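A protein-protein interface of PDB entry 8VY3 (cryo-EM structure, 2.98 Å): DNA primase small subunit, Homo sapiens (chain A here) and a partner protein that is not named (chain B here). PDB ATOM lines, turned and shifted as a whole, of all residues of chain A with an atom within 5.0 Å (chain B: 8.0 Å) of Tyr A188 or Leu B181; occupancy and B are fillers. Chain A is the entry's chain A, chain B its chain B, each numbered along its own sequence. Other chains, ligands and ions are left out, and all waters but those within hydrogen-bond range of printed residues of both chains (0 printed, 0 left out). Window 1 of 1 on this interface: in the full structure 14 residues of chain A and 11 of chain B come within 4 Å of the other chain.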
ATOM      1  N   GLU A 148     -20.772  13.703   3.447  1.00  0.00           N
ATOM      2  CA  GLU A 148     -20.894  14.927   2.664  1.00  0.00           C
ATOM      3  C   GLU A 148     -19.918  14.939   1.494  1.00  0.00           C
ATOM      4  O   GLU A 148     -20.314  15.171   0.347  1.00  0.00           O
ATOM      5  CB  GLU A 148     -20.667  16.140   3.564  1.00  0.00           C
ATOM      6  CG  GLU A 148     -21.915  16.961   3.826  1.00  0.00           C
ATOM      7  CD  GLU A 148     -21.836  17.729   5.130  1.00  0.00           C
ATOM      8  OE1 GLU A 148     -22.900  18.064   5.690  1.00  0.00           O
ATOM      9  OE2 GLU A 148     -20.709  17.997   5.592  1.00  0.00           O
ATOM     10  N   ASP A 149     -18.637  14.695   1.767  1.00  0.00           N
ATOM     11  CA  ASP A 149     -17.623  14.801   0.724  1.00  0.00           C
ATOM     12  C   ASP A 149     -17.737  13.663  -0.282  1.00  0.00           C
ATOM     13  O   ASP A 149     -17.643  13.884  -1.493  1.00  0.00           O
ATOM     14  CB  ASP A 149     -16.232  14.832   1.352  1.00  0.00           C
ATOM     15  CG  ASP A 149     -15.908  16.169   1.977  1.00  0.00           C
ATOM     16  OD1 ASP A 149     -14.767  16.644   1.806  1.00  0.00           O
ATOM     17  OD2 ASP A 149     -16.796  16.750   2.635  1.00  0.00           O
ATOM     18  N   PHE A 150     -17.935  12.436   0.199  1.00  0.00           N
ATOM     19  CA  PHE A 150     -17.944  11.274  -0.679  1.00  0.00           C
ATOM     20  C   PHE A 150     -19.333  10.704  -0.925  1.00  0.00           C
ATOM     21  O   PHE A 150     -19.488   9.869  -1.821  1.00  0.00           O
ATOM     22  CB  PHE A 150     -17.045  10.173  -0.109  1.00  0.00           C
ATOM     23  CG  PHE A 150     -15.591  10.538  -0.067  1.00  0.00           C
ATOM     24  CD1 PHE A 150     -14.995  10.928   1.118  1.00  0.00           C
ATOM     25  CD2 PHE A 150     -14.823  10.500  -1.215  1.00  0.00           C
ATOM     26  CE1 PHE A 150     -13.661  11.263   1.159  1.00  0.00           C
ATOM     27  CE2 PHE A 150     -13.488  10.837  -1.179  1.00  0.00           C
ATOM     28  CZ  PHE A 150     -12.907  11.219   0.009  1.00  0.00           C
ATOM     29  N   GLY A 184      -6.269   6.533  -1.803  1.00  0.00           N
ATOM     30  CA  GLY A 184      -6.535   7.945  -2.026  1.00  0.00           C
ATOM     31  C   GLY A 184      -7.537   8.515  -1.040  1.00  0.00           C
ATOM     32  O   GLY A 184      -7.398   9.653  -0.586  1.00  0.00           O
ATOM     33  N   ILE A 185      -8.563   7.734  -0.698  1.00  0.00           N
ATOM     34  CA  ILE A 185      -9.563   8.180   0.272  1.00  0.00           C
ATOM     35  C   ILE A 185      -8.917   8.387   1.636  1.00  0.00           C
ATOM     36  O   ILE A 185      -9.195   9.369   2.335  1.00  0.00           O
ATOM     37  CB  ILE A 185     -10.728   7.179   0.345  1.00  0.00           C
ATOM     38  CG1 ILE A 185     -11.606   7.294  -0.899  1.00  0.00           C
ATOM     39  CG2 ILE A 185     -11.559   7.412   1.593  1.00  0.00           C
ATOM     40  CD1 ILE A 185     -12.747   6.314  -0.929  1.00  0.00           C
ATOM     41  N   VAL A 186      -8.045   7.460   2.037  1.00  0.00           N
ATOM     42  CA  VAL A 186      -7.330   7.619   3.303  1.00  0.00           C
ATOM     43  C   VAL A 186      -6.414   8.835   3.250  1.00  0.00           C
ATOM     44  O   VAL A 186      -6.254   9.555   4.243  1.00  0.00           O
ATOM     45  CB  VAL A 186      -6.552   6.338   3.650  1.00  0.00           C
ATOM     46  CG1 VAL A 186      -5.836   6.500   4.977  1.00  0.00           C
ATOM     47  CG2 VAL A 186      -7.495   5.161   3.714  1.00  0.00           C
ATOM     48  N   GLU A 187      -5.795   9.081   2.094  1.00  0.00           N
ATOM     49  CA  GLU A 187      -4.957  10.266   1.932  1.00  0.00           C
ATOM     50  C   GLU A 187      -5.766  11.547   2.087  1.00  0.00           C
ATOM     51  O   GLU A 187      -5.281  12.534   2.652  1.00  0.00           O
ATOM     52  CB  GLU A 187      -4.272  10.235   0.566  1.00  0.00           C
ATOM     53  CG  GLU A 187      -2.841   9.744   0.588  1.00  0.00           C
ATOM     54  CD  GLU A 187      -1.992  10.408  -0.476  1.00  0.00           C
ATOM     55  OE1 GLU A 187      -1.815   9.807  -1.556  1.00  0.00           O
ATOM     56  OE2 GLU A 187      -1.505  11.532  -0.235  1.00  0.00           O
ATOM     57  N   TYR A 188      -6.997  11.554   1.575  1.00  0.00           N
ATOM     58  CA  TYR A 188      -7.843  12.740   1.664  1.00  0.00           C
ATOM     59  C   TYR A 188      -8.147  13.097   3.116  1.00  0.00           C
ATOM     60  O   TYR A 188      -8.124  14.273   3.493  1.00  0.00           O
ATOM     61  CB  TYR A 188      -9.137  12.507   0.886  1.00  0.00           C
ATOM     62  CG  TYR A 188     -10.073  13.693   0.841  1.00  0.00           C
ATOM     63  CD1 TYR A 188      -9.819  14.772   0.012  1.00  0.00           C
ATOM     64  CD2 TYR A 188     -11.212  13.730   1.631  1.00  0.00           C
ATOM     65  CE1 TYR A 188     -10.676  15.852  -0.032  1.00  0.00           C
ATOM     66  CE2 TYR A 188     -12.072  14.803   1.595  1.00  0.00           C
ATOM     67  CZ  TYR A 188     -11.799  15.861   0.763  1.00  0.00           C
ATOM     68  OH  TYR A 188     -12.657  16.935   0.726  1.00  0.00           O
ATOM     69  N   LEU A 189      -8.429  12.094   3.943  1.00  0.00           N
ATOM     70  CA  LEU A 189      -8.826  12.306   5.330  1.00  0.00           C
ATOM     71  C   LEU A 189      -7.645  12.411   6.287  1.00  0.00           C
ATOM     72  O   LEU A 189      -7.856  12.697   7.471  1.00  0.00           O
ATOM     73  CB  LEU A 189      -9.752  11.174   5.786  1.00  0.00           C
ATOM     74  CG  LEU A 189     -11.038  10.959   4.990  1.00  0.00           C
ATOM     75  CD1 LEU A 189     -11.852   9.834   5.595  1.00  0.00           C
ATOM     76  CD2 LEU A 189     -11.852  12.237   4.948  1.00  0.00           C
ATOM     77  N   SER A 190      -6.420  12.198   5.818  1.00  0.00           N
ATOM     78  CA  SER A 190      -5.240  12.199   6.672  1.00  0.00           C
ATOM     79  C   SER A 190      -4.660  13.603   6.731  1.00  0.00           C
ATOM     80  O   SER A 190      -4.381  14.209   5.693  1.00  0.00           O
ATOM     81  CB  SER A 190      -4.186  11.213   6.161  1.00  0.00           C
ATOM     82  OG  SER A 190      -4.630   9.876   6.302  1.00  0.00           O
ATOM     83  N   HIS A 209      -8.479  24.376   2.744  1.00  0.00           N
ATOM     84  CA  HIS A 209      -9.490  23.599   2.039  1.00  0.00           C
ATOM     85  C   HIS A 209     -10.768  23.584   2.870  1.00  0.00           C
ATOM     86  O   HIS A 209     -10.698  23.642   4.104  1.00  0.00           O
ATOM     87  CB  HIS A 209      -8.963  22.182   1.784  1.00  0.00           C
ATOM     88  CG  HIS A 209      -9.796  21.376   0.836  1.00  0.00           C
ATOM     89  ND1 HIS A 209     -11.001  20.813   1.190  1.00  0.00           N
ATOM     90  CD2 HIS A 209      -9.586  21.031  -0.457  1.00  0.00           C
ATOM     91  CE1 HIS A 209     -11.502  20.161   0.156  1.00  0.00           C
ATOM     92  NE2 HIS A 209     -10.663  20.277  -0.855  1.00  0.00           N
ATOM     93  N   PHE A 211     -12.628  21.231   3.694  1.00  0.00           N
ATOM     94  CA  PHE A 211     -12.535  20.126   4.642  1.00  0.00           C
ATOM     95  C   PHE A 211     -11.839  20.568   5.924  1.00  0.00           C
ATOM     96  O   PHE A 211     -12.300  20.280   7.035  1.00  0.00           O
ATOM     97  CB  PHE A 211     -11.790  18.953   3.998  1.00  0.00           C
ATOM     98  CG  PHE A 211     -11.644  17.760   4.897  1.00  0.00           C
ATOM     99  CD1 PHE A 211     -10.389  17.320   5.281  1.00  0.00           C
ATOM    100  CD2 PHE A 211     -12.757  17.080   5.356  1.00  0.00           C
ATOM    101  CE1 PHE A 211     -10.248  16.227   6.110  1.00  0.00           C
ATOM    102  CE2 PHE A 211     -12.622  15.984   6.184  1.00  0.00           C
ATOM    103  CZ  PHE A 211     -11.366  15.558   6.561  1.00  0.00           C
ATOM    104  N   GLU B 144     -16.251  28.198  -2.506  1.00  0.00           N
ATOM    105  CA  GLU B 144     -15.702  26.903  -2.121  1.00  0.00           C
ATOM    106  C   GLU B 144     -14.817  26.320  -3.215  1.00  0.00           C
ATOM    107  O   GLU B 144     -13.772  25.733  -2.914  1.00  0.00           O
ATOM    108  CB  GLU B 144     -16.839  25.948  -1.762  1.00  0.00           C
ATOM    109  CG  GLU B 144     -18.075  26.673  -1.245  1.00  0.00           C
ATOM    110  CD  GLU B 144     -19.268  25.762  -1.055  1.00  0.00           C
ATOM    111  OE1 GLU B 144     -20.411  26.238  -1.212  1.00  0.00           O
ATOM    112  OE2 GLU B 144     -19.066  24.576  -0.727  1.00  0.00           O
ATOM    113  N   ILE B 145     -15.210  26.473  -4.482  1.00  0.00           N
ATOM    114  CA  ILE B 145     -14.361  26.024  -5.582  1.00  0.00           C
ATOM    115  C   ILE B 145     -13.051  26.801  -5.599  1.00  0.00           C
ATOM    116  O   ILE B 145     -11.975  26.226  -5.798  1.00  0.00           O
ATOM    117  CB  ILE B 145     -15.110  26.142  -6.922  1.00  0.00           C
ATOM    118  CG1 ILE B 145     -16.217  25.092  -7.010  1.00  0.00           C
ATOM    119  CG2 ILE B 145     -14.152  25.994  -8.087  1.00  0.00           C
ATOM    120  CD1 ILE B 145     -17.175  25.317  -8.154  1.00  0.00           C
ATOM    121  N   SER B 148     -10.883  25.553  -2.651  1.00  0.00           N
ATOM    122  CA  SER B 148     -10.378  24.211  -2.911  1.00  0.00           C
ATOM    123  C   SER B 148      -9.324  24.179  -4.006  1.00  0.00           C
ATOM    124  O   SER B 148      -8.588  23.192  -4.109  1.00  0.00           O
ATOM    125  CB  SER B 148     -11.530  23.282  -3.295  1.00  0.00           C
ATOM    126  OG  SER B 148     -12.555  23.313  -2.321  1.00  0.00           O
ATOM    127  N   ILE B 165     -17.483  15.556 -12.156  1.00  0.00           N
ATOM    128  CA  ILE B 165     -17.169  14.180 -12.534  1.00  0.00           C
ATOM    129  C   ILE B 165     -17.199  13.327 -11.275  1.00  0.00           C
ATOM    130  O   ILE B 165     -17.015  13.836 -10.158  1.00  0.00           O
ATOM    131  CB  ILE B 165     -15.806  14.078 -13.257  1.00  0.00           C
ATOM    132  CG1 ILE B 165     -14.694  14.681 -12.405  1.00  0.00           C
ATOM    133  CG2 ILE B 165     -15.860  14.777 -14.600  1.00  0.00           C
ATOM    134  CD1 ILE B 165     -13.370  14.762 -13.126  1.00  0.00           C
ATOM    135  N   PRO B 166     -17.440  12.024 -11.412  1.00  0.00           N
ATOM    136  CA  PRO B 166     -17.350  11.139 -10.244  1.00  0.00           C
ATOM    137  C   PRO B 166     -15.962  11.203  -9.628  1.00  0.00           C
ATOM    138  O   PRO B 166     -14.959  11.339 -10.331  1.00  0.00           O
ATOM    139  CB  PRO B 166     -17.654   9.757 -10.829  1.00  0.00           C
ATOM    140  CG  PRO B 166     -18.512  10.052 -12.010  1.00  0.00           C
ATOM    141  CD  PRO B 166     -17.943  11.309 -12.597  1.00  0.00           C
ATOM    142  N   PHE B 167     -15.910  11.118  -8.301  1.00  0.00           N
ATOM    143  CA  PHE B 167     -14.669  11.350  -7.573  1.00  0.00           C
ATOM    144  C   PHE B 167     -13.602  10.324  -7.934  1.00  0.00           C
ATOM    145  O   PHE B 167     -12.425  10.675  -8.063  1.00  0.00           O
ATOM    146  CB  PHE B 167     -14.940  11.375  -6.062  1.00  0.00           C
ATOM    147  CG  PHE B 167     -15.072  10.018  -5.428  1.00  0.00           C
ATOM    148  CD1 PHE B 167     -13.982   9.404  -4.834  1.00  0.00           C
ATOM    149  CD2 PHE B 167     -16.290   9.363  -5.413  1.00  0.00           C
ATOM    150  CE1 PHE B 167     -14.107   8.162  -4.246  1.00  0.00           C
ATOM    151  CE2 PHE B 167     -16.416   8.121  -4.827  1.00  0.00           C
ATOM    152  CZ  PHE B 167     -15.324   7.521  -4.245  1.00  0.00           C
ATOM    153  N   ALA B 168     -14.000   9.064  -8.124  1.00  0.00           N
ATOM    154  CA  ALA B 168     -13.030   8.026  -8.456  1.00  0.00           C
ATOM    155  C   ALA B 168     -12.290   8.355  -9.746  1.00  0.00           C
ATOM    156  O   ALA B 168     -11.057   8.259  -9.806  1.00  0.00           O
ATOM    157  CB  ALA B 168     -13.726   6.672  -8.564  1.00  0.00           C
ATOM    158  N   ALA B 170     -11.588  11.144 -10.834  1.00  0.00           N
ATOM    159  CA  ALA B 170     -10.664  12.231 -10.546  1.00  0.00           C
ATOM    160  C   ALA B 170      -9.677  11.863  -9.448  1.00  0.00           C
ATOM    161  O   ALA B 170      -9.235  12.742  -8.701  1.00  0.00           O
ATOM    162  CB  ALA B 170     -11.432  13.496 -10.161  1.00  0.00           C
ATOM    163  N   LEU B 173      -6.478  13.725  -8.557  1.00  0.00           N
ATOM    164  CA  LEU B 173      -6.692  15.079  -8.071  1.00  0.00           C
ATOM    165  C   LEU B 173      -7.203  15.151  -6.642  1.00  0.00           C
ATOM    166  O   LEU B 173      -6.900  16.122  -5.950  1.00  0.00           O
ATOM    167  CB  LEU B 173      -7.679  15.825  -8.978  1.00  0.00           C
ATOM    168  CG  LEU B 173      -7.121  16.405 -10.276  1.00  0.00           C
ATOM    169  CD1 LEU B 173      -8.202  16.448 -11.337  1.00  0.00           C
ATOM    170  CD2 LEU B 173      -6.542  17.785 -10.037  1.00  0.00           C
ATOM    171  N   PHE B 174      -7.961  14.155  -6.172  1.00  0.00           N
ATOM    172  CA  PHE B 174      -8.601  14.316  -4.870  1.00  0.00           C
ATOM    173  C   PHE B 174      -7.773  13.740  -3.732  1.00  0.00           C
ATOM    174  O   PHE B 174      -8.014  14.093  -2.574  1.00  0.00           O
ATOM    175  CB  PHE B 174     -10.017  13.712  -4.888  1.00  0.00           C
ATOM    176  CG  PHE B 174     -10.088  12.250  -4.519  1.00  0.00           C
ATOM    177  CD1 PHE B 174     -10.111  11.842  -3.195  1.00  0.00           C
ATOM    178  CD2 PHE B 174     -10.175  11.287  -5.501  1.00  0.00           C
ATOM    179  CE1 PHE B 174     -10.184  10.507  -2.867  1.00  0.00           C
ATOM    180  CE2 PHE B 174     -10.250   9.948  -5.176  1.00  0.00           C
ATOM    181  CZ  PHE B 174     -10.256   9.560  -3.860  1.00  0.00           C
ATOM    182  N   ARG B 175      -6.809  12.867  -4.027  1.00  0.00           N
ATOM    183  CA  ARG B 175      -5.986  12.308  -2.961  1.00  0.00           C
ATOM    184  C   ARG B 175      -5.000  13.334  -2.423  1.00  0.00           C
ATOM    185  O   ARG B 175      -4.480  13.173  -1.314  1.00  0.00           O
ATOM    186  CB  ARG B 175      -5.258  11.063  -3.459  1.00  0.00           C
ATOM    187  CG  ARG B 175      -3.969  11.334  -4.198  1.00  0.00           C
ATOM    188  CD  ARG B 175      -3.360  10.040  -4.700  1.00  0.00           C
ATOM    189  NE  ARG B 175      -2.110  10.266  -5.414  1.00  0.00           N
ATOM    190  CZ  ARG B 175      -1.502   9.356  -6.161  1.00  0.00           C
ATOM    191  NH1 ARG B 175      -2.005   8.142  -6.318  1.00  0.00           N
ATOM    192  NH2 ARG B 175      -0.361   9.671  -6.766  1.00  0.00           N
ATOM    193  N   GLY B 176      -4.732  14.391  -3.184  1.00  0.00           N
ATOM    194  CA  GLY B 176      -3.899  15.486  -2.740  1.00  0.00           C
ATOM    195  C   GLY B 176      -4.652  16.714  -2.279  1.00  0.00           C
ATOM    196  O   GLY B 176      -4.021  17.754  -2.049  1.00  0.00           O
ATOM    197  N   ARG B 177      -5.975  16.631  -2.137  1.00  0.00           N
ATOM    198  CA  ARG B 177      -6.814  17.750  -1.706  1.00  0.00           C
ATOM    199  C   ARG B 177      -6.637  18.955  -2.633  1.00  0.00           C
ATOM    200  O   ARG B 177      -6.307  20.063  -2.206  1.00  0.00           O
ATOM    201  CB  ARG B 177      -6.521  18.123  -0.249  1.00  0.00           C
ATOM    202  CG  ARG B 177      -7.675  17.872   0.703  1.00  0.00           C
ATOM    203  CD  ARG B 177      -7.236  18.037   2.146  1.00  0.00           C
ATOM    204  NE  ARG B 177      -6.234  17.048   2.521  1.00  0.00           N
ATOM    205  CZ  ARG B 177      -5.348  17.213   3.493  1.00  0.00           C
ATOM    206  NH1 ARG B 177      -5.315  18.318   4.219  1.00  0.00           N
ATOM    207  NH2 ARG B 177      -4.470  16.244   3.742  1.00  0.00           N
ATOM    208  N   LYS B 178      -6.864  18.716  -3.926  1.00  0.00           N
ATOM    209  CA  LYS B 178      -6.682  19.741  -4.949  1.00  0.00           C
ATOM    210  C   LYS B 178      -7.957  20.014  -5.738  1.00  0.00           C
ATOM    211  O   LYS B 178      -7.922  20.766  -6.715  1.00  0.00           O
ATOM    212  CB  LYS B 178      -5.546  19.352  -5.898  1.00  0.00           C
ATOM    213  CG  LYS B 178      -4.160  19.671  -5.360  1.00  0.00           C
ATOM    214  CD  LYS B 178      -3.182  18.545  -5.638  1.00  0.00           C
ATOM    215  CE  LYS B 178      -3.131  18.208  -7.116  1.00  0.00           C
ATOM    216  NZ  LYS B 178      -2.231  17.054  -7.387  1.00  0.00           N
ATOM    217  N   VAL B 179      -9.082  19.421  -5.342  1.00  0.00           N
ATOM    218  CA  VAL B 179     -10.363  19.678  -5.994  1.00  0.00           C
ATOM    219  C   VAL B 179     -11.437  19.740  -4.920  1.00  0.00           C
ATOM    220  O   VAL B 179     -11.266  19.220  -3.818  1.00  0.00           O
ATOM    221  CB  VAL B 179     -10.692  18.601  -7.058  1.00  0.00           C
ATOM    222  CG1 VAL B 179     -10.017  18.931  -8.377  1.00  0.00           C
ATOM    223  CG2 VAL B 179     -10.279  17.224  -6.568  1.00  0.00           C
ATOM    224  N   TYR B 180     -12.555  20.382  -5.247  1.00  0.00           N
ATOM    225  CA  TYR B 180     -13.690  20.454  -4.341  1.00  0.00           C
ATOM    226  C   TYR B 180     -14.561  19.213  -4.492  1.00  0.00           C
ATOM    227  O   TYR B 180     -14.887  18.806  -5.610  1.00  0.00           O
ATOM    228  CB  TYR B 180     -14.508  21.714  -4.615  1.00  0.00           C
ATOM    229  CG  TYR B 180     -15.677  21.894  -3.681  1.00  0.00           C
ATOM    230  CD1 TYR B 180     -15.480  22.203  -2.347  1.00  0.00           C
ATOM    231  CD2 TYR B 180     -16.977  21.749  -4.136  1.00  0.00           C
ATOM    232  CE1 TYR B 180     -16.544  22.363  -1.492  1.00  0.00           C
ATOM    233  CE2 TYR B 180     -18.048  21.906  -3.289  1.00  0.00           C
ATOM    234  CZ  TYR B 180     -17.826  22.212  -1.968  1.00  0.00           C
ATOM    235  OH  TYR B 180     -18.893  22.372  -1.116  1.00  0.00           O
ATOM    236  N   LEU B 181     -14.942  18.617  -3.366  1.00  0.00           N
ATOM    237  CA  LEU B 181     -15.734  17.395  -3.346  1.00  0.00           C
ATOM    238  C   LEU B 181     -17.072  17.643  -2.668  1.00  0.00           C
ATOM    239  O   LEU B 181     -17.134  18.270  -1.607  1.00  0.00           O
ATOM    240  CB  LEU B 181     -14.987  16.272  -2.623  1.00  0.00           C
ATOM    241  CG  LEU B 181     -14.053  15.423  -3.481  1.00  0.00           C
ATOM    242  CD1 LEU B 181     -12.848  14.985  -2.684  1.00  0.00           C
ATOM    243  CD2 LEU B 181     -14.802  14.224  -4.003  1.00  0.00           C
ATOM    244  N   GLU B 182     -18.142  17.143  -3.280  1.00  0.00           N
ATOM    245  CA  GLU B 182     -19.482  17.312  -2.729  1.00  0.00           C
ATOM    246  C   GLU B 182     -20.356  16.164  -3.205  1.00  0.00           C
ATOM    247  O   GLU B 182     -20.745  16.128  -4.376  1.00  0.00           O
ATOM    248  CB  GLU B 182     -20.088  18.655  -3.143  1.00  0.00           C
ATOM    249  CG  GLU B 182     -21.599  18.741  -2.945  1.00  0.00           C
ATOM    250  CD  GLU B 182     -22.025  20.002  -2.222  1.00  0.00           C
ATOM    251  OE1 GLU B 182     -23.204  20.092  -1.820  1.00  0.00           O
ATOM    252  OE2 GLU B 182     -21.180  20.905  -2.056  1.00  0.00           O
ATOM    253  N   ASP B 183     -20.656  15.241  -2.289  1.00  0.00           N
ATOM    254  CA  ASP B 183     -21.548  14.112  -2.522  1.00  0.00           C
ATOM    255  C   ASP B 183     -20.988  13.344  -3.715  1.00  0.00           C
ATOM    256  O   ASP B 183     -21.558  13.368  -4.807  1.00  0.00           O
ATOM    257  CB  ASP B 183     -22.992  14.613  -2.732  1.00  0.00           C
ATOM    258  CG  ASP B 183     -23.955  13.549  -3.288  1.00  0.00           C
ATOM    259  OD1 ASP B 183     -23.559  12.413  -3.621  1.00  0.00           O
ATOM    260  OD2 ASP B 183     -25.158  13.874  -3.387  1.00  0.00           O
ATOM    261  N   GLY B 184     -19.824  12.733  -3.539  1.00  0.00           N
ATOM    262  CA  GLY B 184     -19.285  11.835  -4.543  1.00  0.00           C
ATOM    263  C   GLY B 184     -18.954  12.455  -5.882  1.00  0.00           C
ATOM    264  O   GLY B 184     -18.773  11.729  -6.865  1.00  0.00           O
ATOM    265  N   PHE B 185     -18.864  13.780  -5.951  1.00  0.00           N
ATOM    266  CA  PHE B 185     -18.573  14.459  -7.208  1.00  0.00           C
ATOM    267  C   PHE B 185     -17.468  15.476  -6.984  1.00  0.00           C
ATOM    268  O   PHE B 185     -17.331  16.025  -5.889  1.00  0.00           O
ATOM    269  CB  PHE B 185     -19.812  15.158  -7.782  1.00  0.00           C
ATOM    270  CG  PHE B 185     -20.813  14.221  -8.398  1.00  0.00           C
ATOM    271  CD1 PHE B 185     -20.598  13.684  -9.652  1.00  0.00           C
ATOM    272  CD2 PHE B 185     -21.977  13.898  -7.730  1.00  0.00           C
ATOM    273  CE1 PHE B 185     -21.520  12.830 -10.220  1.00  0.00           C
ATOM    274  CE2 PHE B 185     -22.900  13.045  -8.291  1.00  0.00           C
ATOM    275  CZ  PHE B 185     -22.673  12.511  -9.536  1.00  0.00           C
ATOM    276  N   ALA B 186     -16.683  15.720  -8.028  1.00  0.00           N
ATOM    277  CA  ALA B 186     -15.607  16.694  -8.010  1.00  0.00           C
ATOM    278  C   ALA B 186     -15.830  17.728  -9.104  1.00  0.00           C
ATOM    279  O   ALA B 186     -16.206  17.391 -10.232  1.00  0.00           O
ATOM    280  CB  ALA B 186     -14.247  16.018  -8.198  1.00  0.00           C
ATOM    281  N   TYR B 187     -15.600  18.993  -8.753  1.00  0.00           N
ATOM    282  CA  TYR B 187     -15.734  20.121  -9.667  1.00  0.00           C
ATOM    283  C   TYR B 187     -14.348  20.506 -10.156  1.00  0.00           C
ATOM    284  O   TYR B 187     -13.491  20.900  -9.359  1.00  0.00           O
ATOM    285  CB  TYR B 187     -16.419  21.304  -8.983  1.00  0.00           C
ATOM    286  CG  TYR B 187     -17.838  21.013  -8.556  1.00  0.00           C
ATOM    287  CD1 TYR B 187     -18.109  20.444  -7.323  1.00  0.00           C
ATOM    288  CD2 TYR B 187     -18.905  21.296  -9.395  1.00  0.00           C
ATOM    289  CE1 TYR B 187     -19.403  20.171  -6.932  1.00  0.00           C
ATOM    290  CE2 TYR B 187     -20.201  21.026  -9.014  1.00  0.00           C
ATOM    291  CZ  TYR B 187     -20.446  20.464  -7.781  1.00  0.00           C
ATOM    292  OH  TYR B 187     -21.737  20.194  -7.397  1.00  0.00           O
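Glu B144 touches none of the printed residues of chain A. Ala B170 touches none of the printed residues of chain A. Printed residues of chain A within 4 Å of Arg B175: Gly A184 (3.7 Å) and Glu A187 (3.5 Å). Printed residues of chain A within 4 Å of Val B179: His A209. Leu B181 touches just these residues of chain A: Asp A149 and Tyr A188. Printed residues of chain A within 4 Å of Glu B182: Glu A148 and Asp A149. Of the printed residues of chain A, Gly B184 touches Asp A149 (3.2 Å) and Phe A150 (3.3 Å). The nearest residue of chain B that does not touch Tyr A188 is Arg B175 (4.2 Å). The nearest residue of chain A that does not touch Leu B181 is Phe A150 (4.5 Å).
Glu A148 touches Glu B182. Phe A150 touches Phe B167 (CD2 to CD1, 3.9 Å). Phe A150 touches Phe B174. O of Gly A184 touches CE1 of Phe B174, 3.7 Å away. Gly A184 touches Arg B175. N of Ile A185 touches CE1 of Phe B174, at 3.9 Å. CD1 of Tyr A188 touches O of Phe B174, 3.2 Å away. CE1 of Tyr A188 touches CD1 of Leu B181, at 3.5 Å. His A209 touches Ser B148. O of Arg B177 touches CD2 of His A209 (3.8 Å).
O of Glu A148 lies within hydrogen-bond range of N of Asp B183, at 2.7 Å. The backbone carbonyl oxygen (O) of Asp A149 is in hydrogen-bond range of the backbone NH (N) of Asp B183 (3.4 Å). N of Gly B184 lies within hydrogen-bond range of O of Asp A149 (3.2 Å). O of Phe A150 lies close to N of Gly B184 (3.4 Å). OE1 of Glu A187 lies within salt-bridge range of NE of Arg B175, at 3.9 Å. The guanidinium group (NE) of Arg B177 is in hydrogen-bond range of the backbone carbonyl oxygen (O) of Tyr A188, at 3.5 Å. The guanidinium group (NH2) of Arg B177 is in hydrogen-bond range of the backbone carbonyl oxygen (O) of Ser A190 (2.8 Å). NE2 of His A209 is in hydrogen-bond range of O of Val B179.
Of the 23 printed residues of chain B, 10 touch a printed residue of chain A. Hydrophobic or aromatic side chains of chain B that line the printed part of chain A: Phe B167, Phe B174 and Leu B181. Among the printed residues, 21 pairs touch across the chains.
OG of Ser A190 sits at hydrogen-bond distance from O of Val A186 (2.6 Å). ND1 of His A209 lies within hydrogen-bond range of N of Phe A211. The backbone carbonyl oxygen (O) of Glu B144 sits at hydrogen-bond distance from the side-chain hydroxyl (OG) of Ser B148 (2.8 Å). The backbone NH of Phe B167 sits at hydrogen-bond distance from the backbone carbonyl oxygen of Gly B184 (3.3 Å). The side-chain carboxylate (OE2) of Glu B182 is in hydrogen-bond range of the side-chain hydroxyl (OH) of Tyr B180.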
